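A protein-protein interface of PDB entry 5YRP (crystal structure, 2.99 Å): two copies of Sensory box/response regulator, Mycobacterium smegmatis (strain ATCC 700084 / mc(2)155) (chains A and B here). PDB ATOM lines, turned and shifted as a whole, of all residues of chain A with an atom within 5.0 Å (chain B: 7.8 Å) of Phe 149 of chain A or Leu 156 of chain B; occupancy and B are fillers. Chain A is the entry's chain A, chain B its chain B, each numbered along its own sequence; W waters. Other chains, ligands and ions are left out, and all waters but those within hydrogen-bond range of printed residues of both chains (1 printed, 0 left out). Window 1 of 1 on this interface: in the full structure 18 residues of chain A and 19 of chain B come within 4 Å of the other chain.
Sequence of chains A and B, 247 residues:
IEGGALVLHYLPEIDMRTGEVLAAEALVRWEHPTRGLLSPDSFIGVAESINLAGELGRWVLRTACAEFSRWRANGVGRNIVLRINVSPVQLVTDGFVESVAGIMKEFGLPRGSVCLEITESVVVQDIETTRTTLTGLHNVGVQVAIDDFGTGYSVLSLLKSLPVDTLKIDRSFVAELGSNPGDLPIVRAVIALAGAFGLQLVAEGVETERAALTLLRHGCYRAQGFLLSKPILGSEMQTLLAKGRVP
Of chain B, only Leu 156 comes within 4 Å of Phe 149 of chain A.
Gly 150 of chain A touches just these residues of chain B: Ser 154 (3.4 Å), Val 155 (3.5 Å), Leu 156 (3.4 Å) and Ser 157 (3.1 Å).
Of the printed residues of chain B, Leu 156 of chain A touches Gly 150 (3.8 Å).
Lys 168 of chain A touches none of the printed residues of chain B.
Of the printed residues of chain B, Phe 173 of chain A touches Leu 156 and Ser 157.
Of the printed residues of chain B, Ile 186 of chain A touches Leu 156 and Lys 160.
Of chain A, only Phe 149, Gly 150, Phe 173 and Ile 186 come within 4 Å of Leu 156 of chain B.
Printed residues of chain A within 4 Å of Ser 157 of chain B: Gly 150, Thr 151 and Phe 173.
Ser 161 of chain B touches none of the printed residues of chain A.
Printed residues of chain A within 4 Å of Ala 189 of chain B: Leu 193 (3.5 Å).
The nearest residue of chain B that does not touch Phe 149 of chain A is Ser 157 of chain B (6.1 Å).
The nearest printed residue of chain A that does not touch Ala 189 of chain B is Val 190 of chain A (6.2 Å).
Water W1 bridges N of Val 155 of chain B (3.2 Å) and OE1 of Glu 120 of chain A (3.4 Å).
Phe 149 of chain A touches Leu 156 of chain B, but with the chains exchanged Leu 156 of chain A does not touch Phe 149 of chain B (5.3 Å).
Gly 150 of chain A touches Leu 156 of chain B, and with the chains exchanged Leu 156 of chain A touches Gly 150 of chain B.
Hydrophobic or aromatic side chains of chain B that line the printed part of chain A: Tyr 153, Leu 156 and Ala 189.
Along chain B the printed residues that touch a printed residue of chain A span positions 150 to 189.
Of the 16 printed residues of chain A, 7 touch a printed residue of chain B.
Hydrophobic or aromatic side chains of chain A within 4 Å of the printed part of chain B: Phe 149, Leu 156, Phe 173, Ile 186 and Leu 193.
Among the printed residues, no Asp or Glu carboxylate lies within 4 Å of a Lys or Arg side-chain nitrogen of the other chain.
N of Leu 156 of chain B lies within hydrogen-bond range of O of Gly 150 of chain A, 3.4 Å away.
The backbone carbonyl oxygen of Gly 150 of chain A sits at hydrogen-bond distance from the side-chain hydroxyl of Ser 157 of chain B.
O of Thr 151 of chain A lies within hydrogen-bond range of OG of Ser 154 of chain B (2.5 Å).
Phe 149 of chain A touches Leu 156 of chain B.
O of Gly 150 of chain A touches C of Ser 154 of chain B, at 3.4 Å.
Gly 150 of chain A touches Val 155 of chain B.
Tyr 153 of chain B touches Thr 151 of chain A.
Thr 151 of chain A touches Ser 157 of chain B.
CZ of Phe 173 of chain A touches CB of Leu 156 of chain B (3.7 Å).
Ser 157 of chain B touches Phe 173 of chain A.
Ile 186 of chain A touches Leu 156 of chain B.
Ile 186 of chain A touches Lys 160 of chain B.
CD1 of Leu 193 of chain A touches CB of Ala 189 of chain B, at 3.5 Å.
The backbone NH (N) of Gly 150 of chain A sits at hydrogen-bond distance from the side-chain carboxylate (OE1) of Glu 120 of chain A, at 2.5 Å.
The backbone carbonyl oxygen (O) of Asp 148 of chain A lies within hydrogen-bond range of the side-chain hydroxyl (OG1) of Thr 151 of chain A (2.6 Å).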
ATOM      1  N   GLU A 120      23.904 -17.866   1.847  1.00  0.00           N
ATOM      2  CA  GLU A 120      22.731 -16.996   1.857  1.00  0.00           C
ATOM      3  C   GLU A 120      22.124 -16.857   3.259  1.00  0.00           C
ATOM      4  O   GLU A 120      21.627 -15.793   3.619  1.00  0.00           O
ATOM      5  CB  GLU A 120      21.682 -17.507   0.864  1.00  0.00           C
ATOM      6  CG  GLU A 120      20.525 -16.542   0.661  1.00  0.00           C
ATOM      7  CD  GLU A 120      19.487 -17.032  -0.323  1.00  0.00           C
ATOM      8  OE1 GLU A 120      19.450 -18.250  -0.624  1.00  0.00           O
ATOM      9  OE2 GLU A 120      18.691 -16.187  -0.786  1.00  0.00           O
ATOM     10  N   ILE A 146      27.267 -14.506  -3.275  1.00  0.00           N
ATOM     11  CA  ILE A 146      26.220 -15.207  -2.540  1.00  0.00           C
ATOM     12  C   ILE A 146      26.062 -16.631  -3.080  1.00  0.00           C
ATOM     13  O   ILE A 146      25.488 -16.878  -4.144  1.00  0.00           O
ATOM     14  CB  ILE A 146      24.881 -14.452  -2.586  1.00  0.00           C
ATOM     15  CG1 ILE A 146      25.003 -13.106  -1.853  1.00  0.00           C
ATOM     16  CG2 ILE A 146      23.756 -15.287  -1.982  1.00  0.00           C
ATOM     17  CD1 ILE A 146      25.265 -13.196  -0.358  1.00  0.00           C
ATOM     18  N   ASP A 147      26.598 -17.540  -2.282  1.00  0.00           N
ATOM     19  CA  ASP A 147      26.669 -18.974  -2.497  1.00  0.00           C
ATOM     20  C   ASP A 147      25.341 -19.632  -2.205  1.00  0.00           C
ATOM     21  O   ASP A 147      24.589 -19.138  -1.360  1.00  0.00           O
ATOM     22  CB  ASP A 147      27.645 -19.503  -1.440  1.00  0.00           C
ATOM     23  CG  ASP A 147      28.515 -20.623  -1.922  1.00  0.00           C
ATOM     24  OD1 ASP A 147      29.338 -21.087  -1.103  1.00  0.00           O
ATOM     25  OD2 ASP A 147      28.403 -21.048  -3.093  1.00  0.00           O
ATOM     26  N   ASP A 148      25.066 -20.763  -2.851  1.00  0.00           N
ATOM     27  CA  ASP A 148      23.897 -21.567  -2.495  1.00  0.00           C
ATOM     28  C   ASP A 148      22.667 -20.676  -2.332  1.00  0.00           C
ATOM     29  O   ASP A 148      22.054 -20.613  -1.259  1.00  0.00           O
ATOM     30  CB  ASP A 148      24.165 -22.333  -1.188  1.00  0.00           C
ATOM     31  CG  ASP A 148      25.155 -23.472  -1.362  1.00  0.00           C
ATOM     32  OD1 ASP A 148      25.453 -23.860  -2.514  1.00  0.00           O
ATOM     33  OD2 ASP A 148      25.635 -23.989  -0.332  1.00  0.00           O
ATOM     34  N   PHE A 149      22.337 -19.963  -3.401  1.00  0.00           N
ATOM     35  CA  PHE A 149      21.229 -19.012  -3.379  1.00  0.00           C
ATOM     36  C   PHE A 149      19.895 -19.699  -3.640  1.00  0.00           C
ATOM     37  O   PHE A 149      19.768 -20.472  -4.584  1.00  0.00           O
ATOM     38  CB  PHE A 149      21.448 -17.925  -4.422  1.00  0.00           C
ATOM     39  CG  PHE A 149      20.348 -16.908  -4.468  1.00  0.00           C
ATOM     40  CD1 PHE A 149      20.324 -15.856  -3.570  1.00  0.00           C
ATOM     41  CD2 PHE A 149      19.332 -17.006  -5.404  1.00  0.00           C
ATOM     42  CE1 PHE A 149      19.308 -14.914  -3.607  1.00  0.00           C
ATOM     43  CE2 PHE A 149      18.314 -16.070  -5.447  1.00  0.00           C
ATOM     44  CZ  PHE A 149      18.299 -15.023  -4.545  1.00  0.00           C
ATOM     45  N   GLY A 150      18.900 -19.383  -2.814  1.00  0.00           N
ATOM     46  CA  GLY A 150      17.580 -20.011  -2.885  1.00  0.00           C
ATOM     47  C   GLY A 150      17.454 -21.281  -2.063  1.00  0.00           C
ATOM     48  O   GLY A 150      16.397 -21.913  -2.063  1.00  0.00           O
ATOM     49  N   THR A 151      18.525 -21.654  -1.363  1.00  0.00           N
ATOM     50  CA  THR A 151      18.537 -22.866  -0.540  1.00  0.00           C
ATOM     51  C   THR A 151      18.438 -22.554   0.939  1.00  0.00           C
ATOM     52  O   THR A 151      17.746 -23.248   1.674  1.00  0.00           O
ATOM     53  CB  THR A 151      19.827 -23.670  -0.733  1.00  0.00           C
ATOM     54  OG1 THR A 151      20.953 -22.840  -0.430  1.00  0.00           O
ATOM     55  CG2 THR A 151      19.929 -24.187  -2.152  1.00  0.00           C
ATOM     56  N   LEU A 156      16.264 -12.320  -0.579  1.00  0.00           N
ATOM     57  CA  LEU A 156      15.505 -11.561  -1.581  1.00  0.00           C
ATOM     58  C   LEU A 156      15.107 -10.181  -1.067  1.00  0.00           C
ATOM     59  O   LEU A 156      15.226  -9.190  -1.789  1.00  0.00           O
ATOM     60  CB  LEU A 156      14.256 -12.327  -2.023  1.00  0.00           C
ATOM     61  CG  LEU A 156      14.475 -13.520  -2.953  1.00  0.00           C
ATOM     62  CD1 LEU A 156      13.157 -14.221  -3.216  1.00  0.00           C
ATOM     63  CD2 LEU A 156      15.108 -13.103  -4.268  1.00  0.00           C
ATOM     64  N   LEU A 159      18.494  -8.111  -1.088  1.00  0.00           N
ATOM     65  CA  LEU A 159      19.392  -8.134  -2.253  1.00  0.00           C
ATOM     66  C   LEU A 159      19.595  -6.743  -2.835  1.00  0.00           C
ATOM     67  O   LEU A 159      20.710  -6.370  -3.197  1.00  0.00           O
ATOM     68  CB  LEU A 159      18.858  -9.049  -3.358  1.00  0.00           C
ATOM     69  CG  LEU A 159      19.171 -10.545  -3.296  1.00  0.00           C
ATOM     70  CD1 LEU A 159      18.654 -11.211  -4.564  1.00  0.00           C
ATOM     71  CD2 LEU A 159      20.657 -10.835  -3.120  1.00  0.00           C
ATOM     72  N   LEU A 167      26.513 -13.565  -7.770  1.00  0.00           N
ATOM     73  CA  LEU A 167      25.425 -14.415  -7.316  1.00  0.00           C
ATOM     74  C   LEU A 167      25.568 -15.797  -7.958  1.00  0.00           C
ATOM     75  O   LEU A 167      25.723 -15.910  -9.176  1.00  0.00           O
ATOM     76  CB  LEU A 167      24.087 -13.773  -7.682  1.00  0.00           C
ATOM     77  CG  LEU A 167      22.813 -14.396  -7.116  1.00  0.00           C
ATOM     78  CD1 LEU A 167      22.850 -14.472  -5.601  1.00  0.00           C
ATOM     79  CD2 LEU A 167      21.604 -13.596  -7.564  1.00  0.00           C
ATOM     80  N   LYS A 168      25.534 -16.840  -7.132  1.00  0.00           N
ATOM     81  CA  LYS A 168      25.745 -18.210  -7.606  1.00  0.00           C
ATOM     82  C   LYS A 168      24.458 -19.018  -7.696  1.00  0.00           C
ATOM     83  O   LYS A 168      23.635 -18.998  -6.777  1.00  0.00           O
ATOM     84  CB  LYS A 168      26.725 -18.948  -6.699  1.00  0.00           C
ATOM     85  CG  LYS A 168      28.136 -18.390  -6.732  1.00  0.00           C
ATOM     86  CD  LYS A 168      29.157 -19.430  -6.302  1.00  0.00           C
ATOM     87  CE  LYS A 168      30.576 -19.001  -6.634  1.00  0.00           C
ATOM     88  NZ  LYS A 168      31.510 -20.162  -6.619  1.00  0.00           N
ATOM     89  N   ASP A 170      22.781 -22.311  -7.268  1.00  0.00           N
ATOM     90  CA  ASP A 170      23.034 -23.525  -6.477  1.00  0.00           C
ATOM     91  C   ASP A 170      23.046 -24.809  -7.317  1.00  0.00           C
ATOM     92  O   ASP A 170      22.386 -24.894  -8.356  1.00  0.00           O
ATOM     93  CB  ASP A 170      21.987 -23.645  -5.363  1.00  0.00           C
ATOM     94  CG  ASP A 170      22.249 -24.813  -4.431  1.00  0.00           C
ATOM     95  OD1 ASP A 170      23.095 -24.677  -3.525  1.00  0.00           O
ATOM     96  OD2 ASP A 170      21.592 -25.867  -4.592  1.00  0.00           O
ATOM     97  N   PHE A 173      19.618 -26.597  -8.622  1.00  0.00           N
ATOM     98  CA  PHE A 173      18.915 -26.054  -9.794  1.00  0.00           C
ATOM     99  C   PHE A 173      19.655 -26.316 -11.104  1.00  0.00           C
ATOM    100  O   PHE A 173      19.085 -26.167 -12.181  1.00  0.00           O
ATOM    101  CB  PHE A 173      18.685 -24.549  -9.637  1.00  0.00           C
ATOM    102  CG  PHE A 173      18.132 -24.157  -8.297  1.00  0.00           C
ATOM    103  CD1 PHE A 173      17.064 -24.849  -7.739  1.00  0.00           C
ATOM    104  CD2 PHE A 173      18.680 -23.102  -7.594  1.00  0.00           C
ATOM    105  CE1 PHE A 173      16.558 -24.494  -6.504  1.00  0.00           C
ATOM    106  CE2 PHE A 173      18.176 -22.740  -6.361  1.00  0.00           C
ATOM    107  CZ  PHE A 173      17.114 -23.435  -5.816  1.00  0.00           C
ATOM    108  N   ILE A 186      13.445 -21.462 -12.235  1.00  0.00           N
ATOM    109  CA  ILE A 186      14.199 -20.936 -11.101  1.00  0.00           C
ATOM    110  C   ILE A 186      15.514 -20.344 -11.589  1.00  0.00           C
ATOM    111  O   ILE A 186      15.913 -19.257 -11.170  1.00  0.00           O
ATOM    112  CB  ILE A 186      14.453 -22.029 -10.040  1.00  0.00           C
ATOM    113  CG1 ILE A 186      13.116 -22.467  -9.425  1.00  0.00           C
ATOM    114  CG2 ILE A 186      15.385 -21.516  -8.951  1.00  0.00           C
ATOM    115  CD1 ILE A 186      13.187 -23.723  -8.583  1.00  0.00           C
ATOM    116  N   VAL A 190      16.552 -16.295 -11.327  1.00  0.00           N
ATOM    117  CA  VAL A 190      17.777 -15.792 -10.682  1.00  0.00           C
ATOM    118  C   VAL A 190      18.661 -14.971 -11.635  1.00  0.00           C
ATOM    119  O   VAL A 190      19.303 -14.003 -11.216  1.00  0.00           O
ATOM    120  CB  VAL A 190      18.593 -16.940 -10.030  1.00  0.00           C
ATOM    121  CG1 VAL A 190      19.130 -17.905 -11.076  1.00  0.00           C
ATOM    122  CG2 VAL A 190      19.727 -16.392  -9.171  1.00  0.00           C
ATOM    123  N   LEU A 193      17.320 -11.462 -11.776  1.00  0.00           N
ATOM    124  CA  LEU A 193      17.661 -10.737 -10.547  1.00  0.00           C
ATOM    125  C   LEU A 193      19.074 -10.167 -10.624  1.00  0.00           C
ATOM    126  O   LEU A 193      19.291  -8.975 -10.406  1.00  0.00           O
ATOM    127  CB  LEU A 193      17.537 -11.639  -9.315  1.00  0.00           C
ATOM    128  CG  LEU A 193      16.131 -11.773  -8.721  1.00  0.00           C
ATOM    129  CD1 LEU A 193      15.253 -12.656  -9.588  1.00  0.00           C
ATOM    130  CD2 LEU A 193      16.185 -12.338  -7.313  1.00  0.00           C
ATOM    131  N   GLU B 120       6.823 -20.302   4.657  1.00  0.00           N
ATOM    132  CA  GLU B 120       7.939 -20.716   3.812  1.00  0.00           C
ATOM    133  C   GLU B 120       9.044 -21.347   4.662  1.00  0.00           C
ATOM    134  O   GLU B 120       9.801 -22.189   4.180  1.00  0.00           O
ATOM    135  CB  GLU B 120       8.467 -19.519   3.005  1.00  0.00           C
ATOM    136  CG  GLU B 120       9.594 -19.831   2.024  1.00  0.00           C
ATOM    137  CD  GLU B 120       9.242 -20.903   1.002  1.00  0.00           C
ATOM    138  OE1 GLU B 120       8.052 -21.082   0.681  1.00  0.00           O
ATOM    139  OE2 GLU B 120      10.165 -21.577   0.506  1.00  0.00           O
ATOM    140  N   PHE B 149       5.992 -15.323   1.191  1.00  0.00           N
ATOM    141  CA  PHE B 149       6.933 -15.852   0.203  1.00  0.00           C
ATOM    142  C   PHE B 149       8.161 -14.952   0.066  1.00  0.00           C
ATOM    143  O   PHE B 149       8.044 -13.727   0.107  1.00  0.00           O
ATOM    144  CB  PHE B 149       6.249 -16.020  -1.154  1.00  0.00           C
ATOM    145  CG  PHE B 149       7.137 -16.607  -2.213  1.00  0.00           C
ATOM    146  CD1 PHE B 149       7.540 -17.932  -2.141  1.00  0.00           C
ATOM    147  CD2 PHE B 149       7.567 -15.839  -3.285  1.00  0.00           C
ATOM    148  CE1 PHE B 149       8.356 -18.482  -3.115  1.00  0.00           C
ATOM    149  CE2 PHE B 149       8.387 -16.383  -4.261  1.00  0.00           C
ATOM    150  CZ  PHE B 149       8.783 -17.705  -4.176  1.00  0.00           C
ATOM    151  N   GLY B 150       9.331 -15.573  -0.074  1.00  0.00           N
ATOM    152  CA  GLY B 150      10.587 -14.848  -0.279  1.00  0.00           C
ATOM    153  C   GLY B 150      11.348 -14.500   0.991  1.00  0.00           C
ATOM    154  O   GLY B 150      12.431 -13.912   0.928  1.00  0.00           O
ATOM    155  N   GLY B 152      11.376 -16.928   3.847  1.00  0.00           N
ATOM    156  CA  GLY B 152      11.617 -18.139   4.625  1.00  0.00           C
ATOM    157  C   GLY B 152      12.912 -18.858   4.296  1.00  0.00           C
ATOM    158  O   GLY B 152      13.912 -18.234   3.932  1.00  0.00           O
ATOM    159  N   TYR B 153      12.875 -20.181   4.442  1.00  0.00           N
ATOM    160  CA  TYR B 153      14.030 -21.046   4.204  1.00  0.00           C
ATOM    161  C   TYR B 153      13.792 -21.862   2.932  1.00  0.00           C
ATOM    162  O   TYR B 153      12.694 -22.367   2.711  1.00  0.00           O
ATOM    163  CB  TYR B 153      14.272 -21.966   5.419  1.00  0.00           C
ATOM    164  CG  TYR B 153      15.383 -22.996   5.239  1.00  0.00           C
ATOM    165  CD1 TYR B 153      16.717 -22.678   5.504  1.00  0.00           C
ATOM    166  CD2 TYR B 153      15.094 -24.297   4.808  1.00  0.00           C
ATOM    167  CE1 TYR B 153      17.730 -23.620   5.339  1.00  0.00           C
ATOM    168  CE2 TYR B 153      16.097 -25.243   4.642  1.00  0.00           C
ATOM    169  CZ  TYR B 153      17.409 -24.901   4.908  1.00  0.00           C
ATOM    170  OH  TYR B 153      18.394 -25.845   4.740  1.00  0.00           O
ATOM    171  N   SER B 154      14.831 -21.981   2.108  1.00  0.00           N
ATOM    172  CA  SER B 154      14.774 -22.735   0.848  1.00  0.00           C
ATOM    173  C   SER B 154      13.651 -22.233  -0.064  1.00  0.00           C
ATOM    174  O   SER B 154      12.901 -23.019  -0.639  1.00  0.00           O
ATOM    175  CB  SER B 154      14.631 -24.242   1.120  1.00  0.00           C
ATOM    176  OG  SER B 154      15.855 -24.810   1.553  1.00  0.00           O
ATOM    177  N   VAL B 155      13.561 -20.915  -0.207  1.00  0.00           N
ATOM    178  CA  VAL B 155      12.463 -20.278  -0.937  1.00  0.00           C
ATOM    179  C   VAL B 155      12.256 -20.871  -2.333  1.00  0.00           C
ATOM    180  O   VAL B 155      11.160 -21.329  -2.672  1.00  0.00           O
ATOM    181  CB  VAL B 155      12.677 -18.759  -1.032  1.00  0.00           C
ATOM    182  CG1 VAL B 155      11.724 -18.132  -2.042  1.00  0.00           C
ATOM    183  CG2 VAL B 155      12.473 -18.124   0.333  1.00  0.00           C
ATOM    184  N   LEU B 156      13.316 -20.856  -3.129  1.00  0.00           N
ATOM    185  CA  LEU B 156      13.263 -21.337  -4.513  1.00  0.00           C
ATOM    186  C   LEU B 156      13.170 -22.863  -4.614  1.00  0.00           C
ATOM    187  O   LEU B 156      12.480 -23.392  -5.488  1.00  0.00           O
ATOM    188  CB  LEU B 156      14.480 -20.830  -5.293  1.00  0.00           C
ATOM    189  CG  LEU B 156      14.653 -19.306  -5.338  1.00  0.00           C
ATOM    190  CD1 LEU B 156      15.882 -18.920  -6.146  1.00  0.00           C
ATOM    191  CD2 LEU B 156      13.424 -18.621  -5.917  1.00  0.00           C
ATOM    192  N   SER B 157      13.868 -23.560  -3.722  1.00  0.00           N
ATOM    193  CA  SER B 157      13.854 -25.023  -3.686  1.00  0.00           C
ATOM    194  C   SER B 157      12.448 -25.580  -3.495  1.00  0.00           C
ATOM    195  O   SER B 157      12.052 -26.528  -4.178  1.00  0.00           O
ATOM    196  CB  SER B 157      14.753 -25.530  -2.559  1.00  0.00           C
ATOM    197  OG  SER B 157      16.025 -24.919  -2.622  1.00  0.00           O
ATOM    198  N   LEU B 158      11.701 -24.985  -2.568  1.00  0.00           N
ATOM    199  CA  LEU B 158      10.365 -25.471  -2.223  1.00  0.00           C
ATOM    200  C   LEU B 158       9.438 -25.531  -3.436  1.00  0.00           C
ATOM    201  O   LEU B 158       8.637 -26.458  -3.562  1.00  0.00           O
ATOM    202  CB  LEU B 158       9.735 -24.636  -1.096  1.00  0.00           C
ATOM    203  CG  LEU B 158       9.923 -25.211   0.319  1.00  0.00           C
ATOM    204  CD1 LEU B 158      11.342 -25.026   0.827  1.00  0.00           C
ATOM    205  CD2 LEU B 158       8.942 -24.593   1.306  1.00  0.00           C
ATOM    206  N   LEU B 159       9.569 -24.558  -4.333  1.00  0.00           N
ATOM    207  CA  LEU B 159       8.758 -24.517  -5.552  1.00  0.00           C
ATOM    208  C   LEU B 159       8.842 -25.798  -6.387  1.00  0.00           C
ATOM    209  O   LEU B 159       7.851 -26.221  -6.986  1.00  0.00           O
ATOM    210  CB  LEU B 159       9.149 -23.315  -6.414  1.00  0.00           C
ATOM    211  CG  LEU B 159       8.869 -21.930  -5.827  1.00  0.00           C
ATOM    212  CD1 LEU B 159       9.278 -20.858  -6.823  1.00  0.00           C
ATOM    213  CD2 LEU B 159       7.403 -21.760  -5.445  1.00  0.00           C
ATOM    214  N   LYS B 160      10.016 -26.416  -6.418  1.00  0.00           N
ATOM    215  CA  LYS B 160      10.211 -27.648  -7.181  1.00  0.00           C
ATOM    216  C   LYS B 160       9.498 -28.834  -6.545  1.00  0.00           C
ATOM    217  O   LYS B 160       8.744 -29.554  -7.206  1.00  0.00           O
ATOM    218  CB  LYS B 160      11.693 -27.985  -7.287  1.00  0.00           C
ATOM    219  CG  LYS B 160      12.538 -26.916  -7.951  1.00  0.00           C
ATOM    220  CD  LYS B 160      13.767 -27.518  -8.614  1.00  0.00           C
ATOM    221  CE  LYS B 160      14.595 -28.361  -7.657  1.00  0.00           C
ATOM    222  NZ  LYS B 160      15.872 -28.797  -8.277  1.00  0.00           N
ATOM    223  N   SER B 161       9.757 -29.025  -5.256  1.00  0.00           N
ATOM    224  CA  SER B 161       9.329 -30.222  -4.535  1.00  0.00           C
ATOM    225  C   SER B 161       7.846 -30.227  -4.170  1.00  0.00           C
ATOM    226  O   SER B 161       7.140 -31.203  -4.435  1.00  0.00           O
ATOM    227  CB  SER B 161      10.164 -30.388  -3.265  1.00  0.00           C
ATOM    228  OG  SER B 161      10.100 -29.224  -2.464  1.00  0.00           O
ATOM    229  N   ALA B 189       9.985 -10.862 -11.153  1.00  0.00           N
ATOM    230  CA  ALA B 189      10.560 -12.210 -11.165  1.00  0.00           C
ATOM    231  C   ALA B 189       9.716 -13.234 -10.398  1.00  0.00           C
ATOM    232  O   ALA B 189       9.619 -14.393 -10.801  1.00  0.00           O
ATOM    233  CB  ALA B 189      11.978 -12.174 -10.613  1.00  0.00           C
ATOM    234  N   VAL B 190       9.117 -12.810  -9.290  1.00  0.00           N
ATOM    235  CA  VAL B 190       8.262 -13.694  -8.498  1.00  0.00           C
ATOM    236  C   VAL B 190       6.990 -14.039  -9.274  1.00  0.00           C
ATOM    237  O   VAL B 190       6.536 -15.185  -9.260  1.00  0.00           O
ATOM    238  CB  VAL B 190       7.885 -13.060  -7.140  1.00  0.00           C
ATOM    239  CG1 VAL B 190       6.860 -13.916  -6.399  1.00  0.00           C
ATOM    240  CG2 VAL B 190       9.124 -12.858  -6.280  1.00  0.00           C
ATOM    241  N   LEU B 193       7.769 -16.628 -11.841  1.00  0.00           N
ATOM    242  CA  LEU B 193       7.834 -17.938 -11.186  1.00  0.00           C
ATOM    243  C   LEU B 193       6.451 -18.538 -11.005  1.00  0.00           C
ATOM    244  O   LEU B 193       6.209 -19.678 -11.397  1.00  0.00           O
ATOM    245  CB  LEU B 193       8.517 -17.831  -9.820  1.00  0.00           C
ATOM    246  CG  LEU B 193      10.043 -17.786  -9.831  1.00  0.00           C
ATOM    247  CD1 LEU B 193      10.577 -17.271  -8.505  1.00  0.00           C
ATOM    248  CD2 LEU B 193      10.606 -19.165 -10.143  1.00  0.00           C
ATOM    249  N   PHE B 197       5.232 -21.786 -12.721  1.00  0.00           N
ATOM    250  CA  PHE B 197       4.912 -22.961 -11.887  1.00  0.00           C
ATOM    251  C   PHE B 197       3.413 -23.272 -11.791  1.00  0.00           C
ATOM    252  O   PHE B 197       3.006 -24.165 -11.036  1.00  0.00           O
ATOM    253  CB  PHE B 197       5.502 -22.800 -10.482  1.00  0.00           C
ATOM    254  CG  PHE B 197       6.898 -23.323 -10.358  1.00  0.00           C
ATOM    255  CD1 PHE B 197       7.124 -24.648 -10.021  1.00  0.00           C
ATOM    256  CD2 PHE B 197       7.989 -22.497 -10.597  1.00  0.00           C
ATOM    257  CE1 PHE B 197       8.413 -25.142  -9.917  1.00  0.00           C
ATOM    258  CE2 PHE B 197       9.279 -22.984 -10.494  1.00  0.00           C
ATOM    259  CZ  PHE B 197       9.491 -24.309 -10.154  1.00  0.00           C
HETATM  260  O   HOH W   1      16.224 -19.104   0.080  1.00  0.00           O
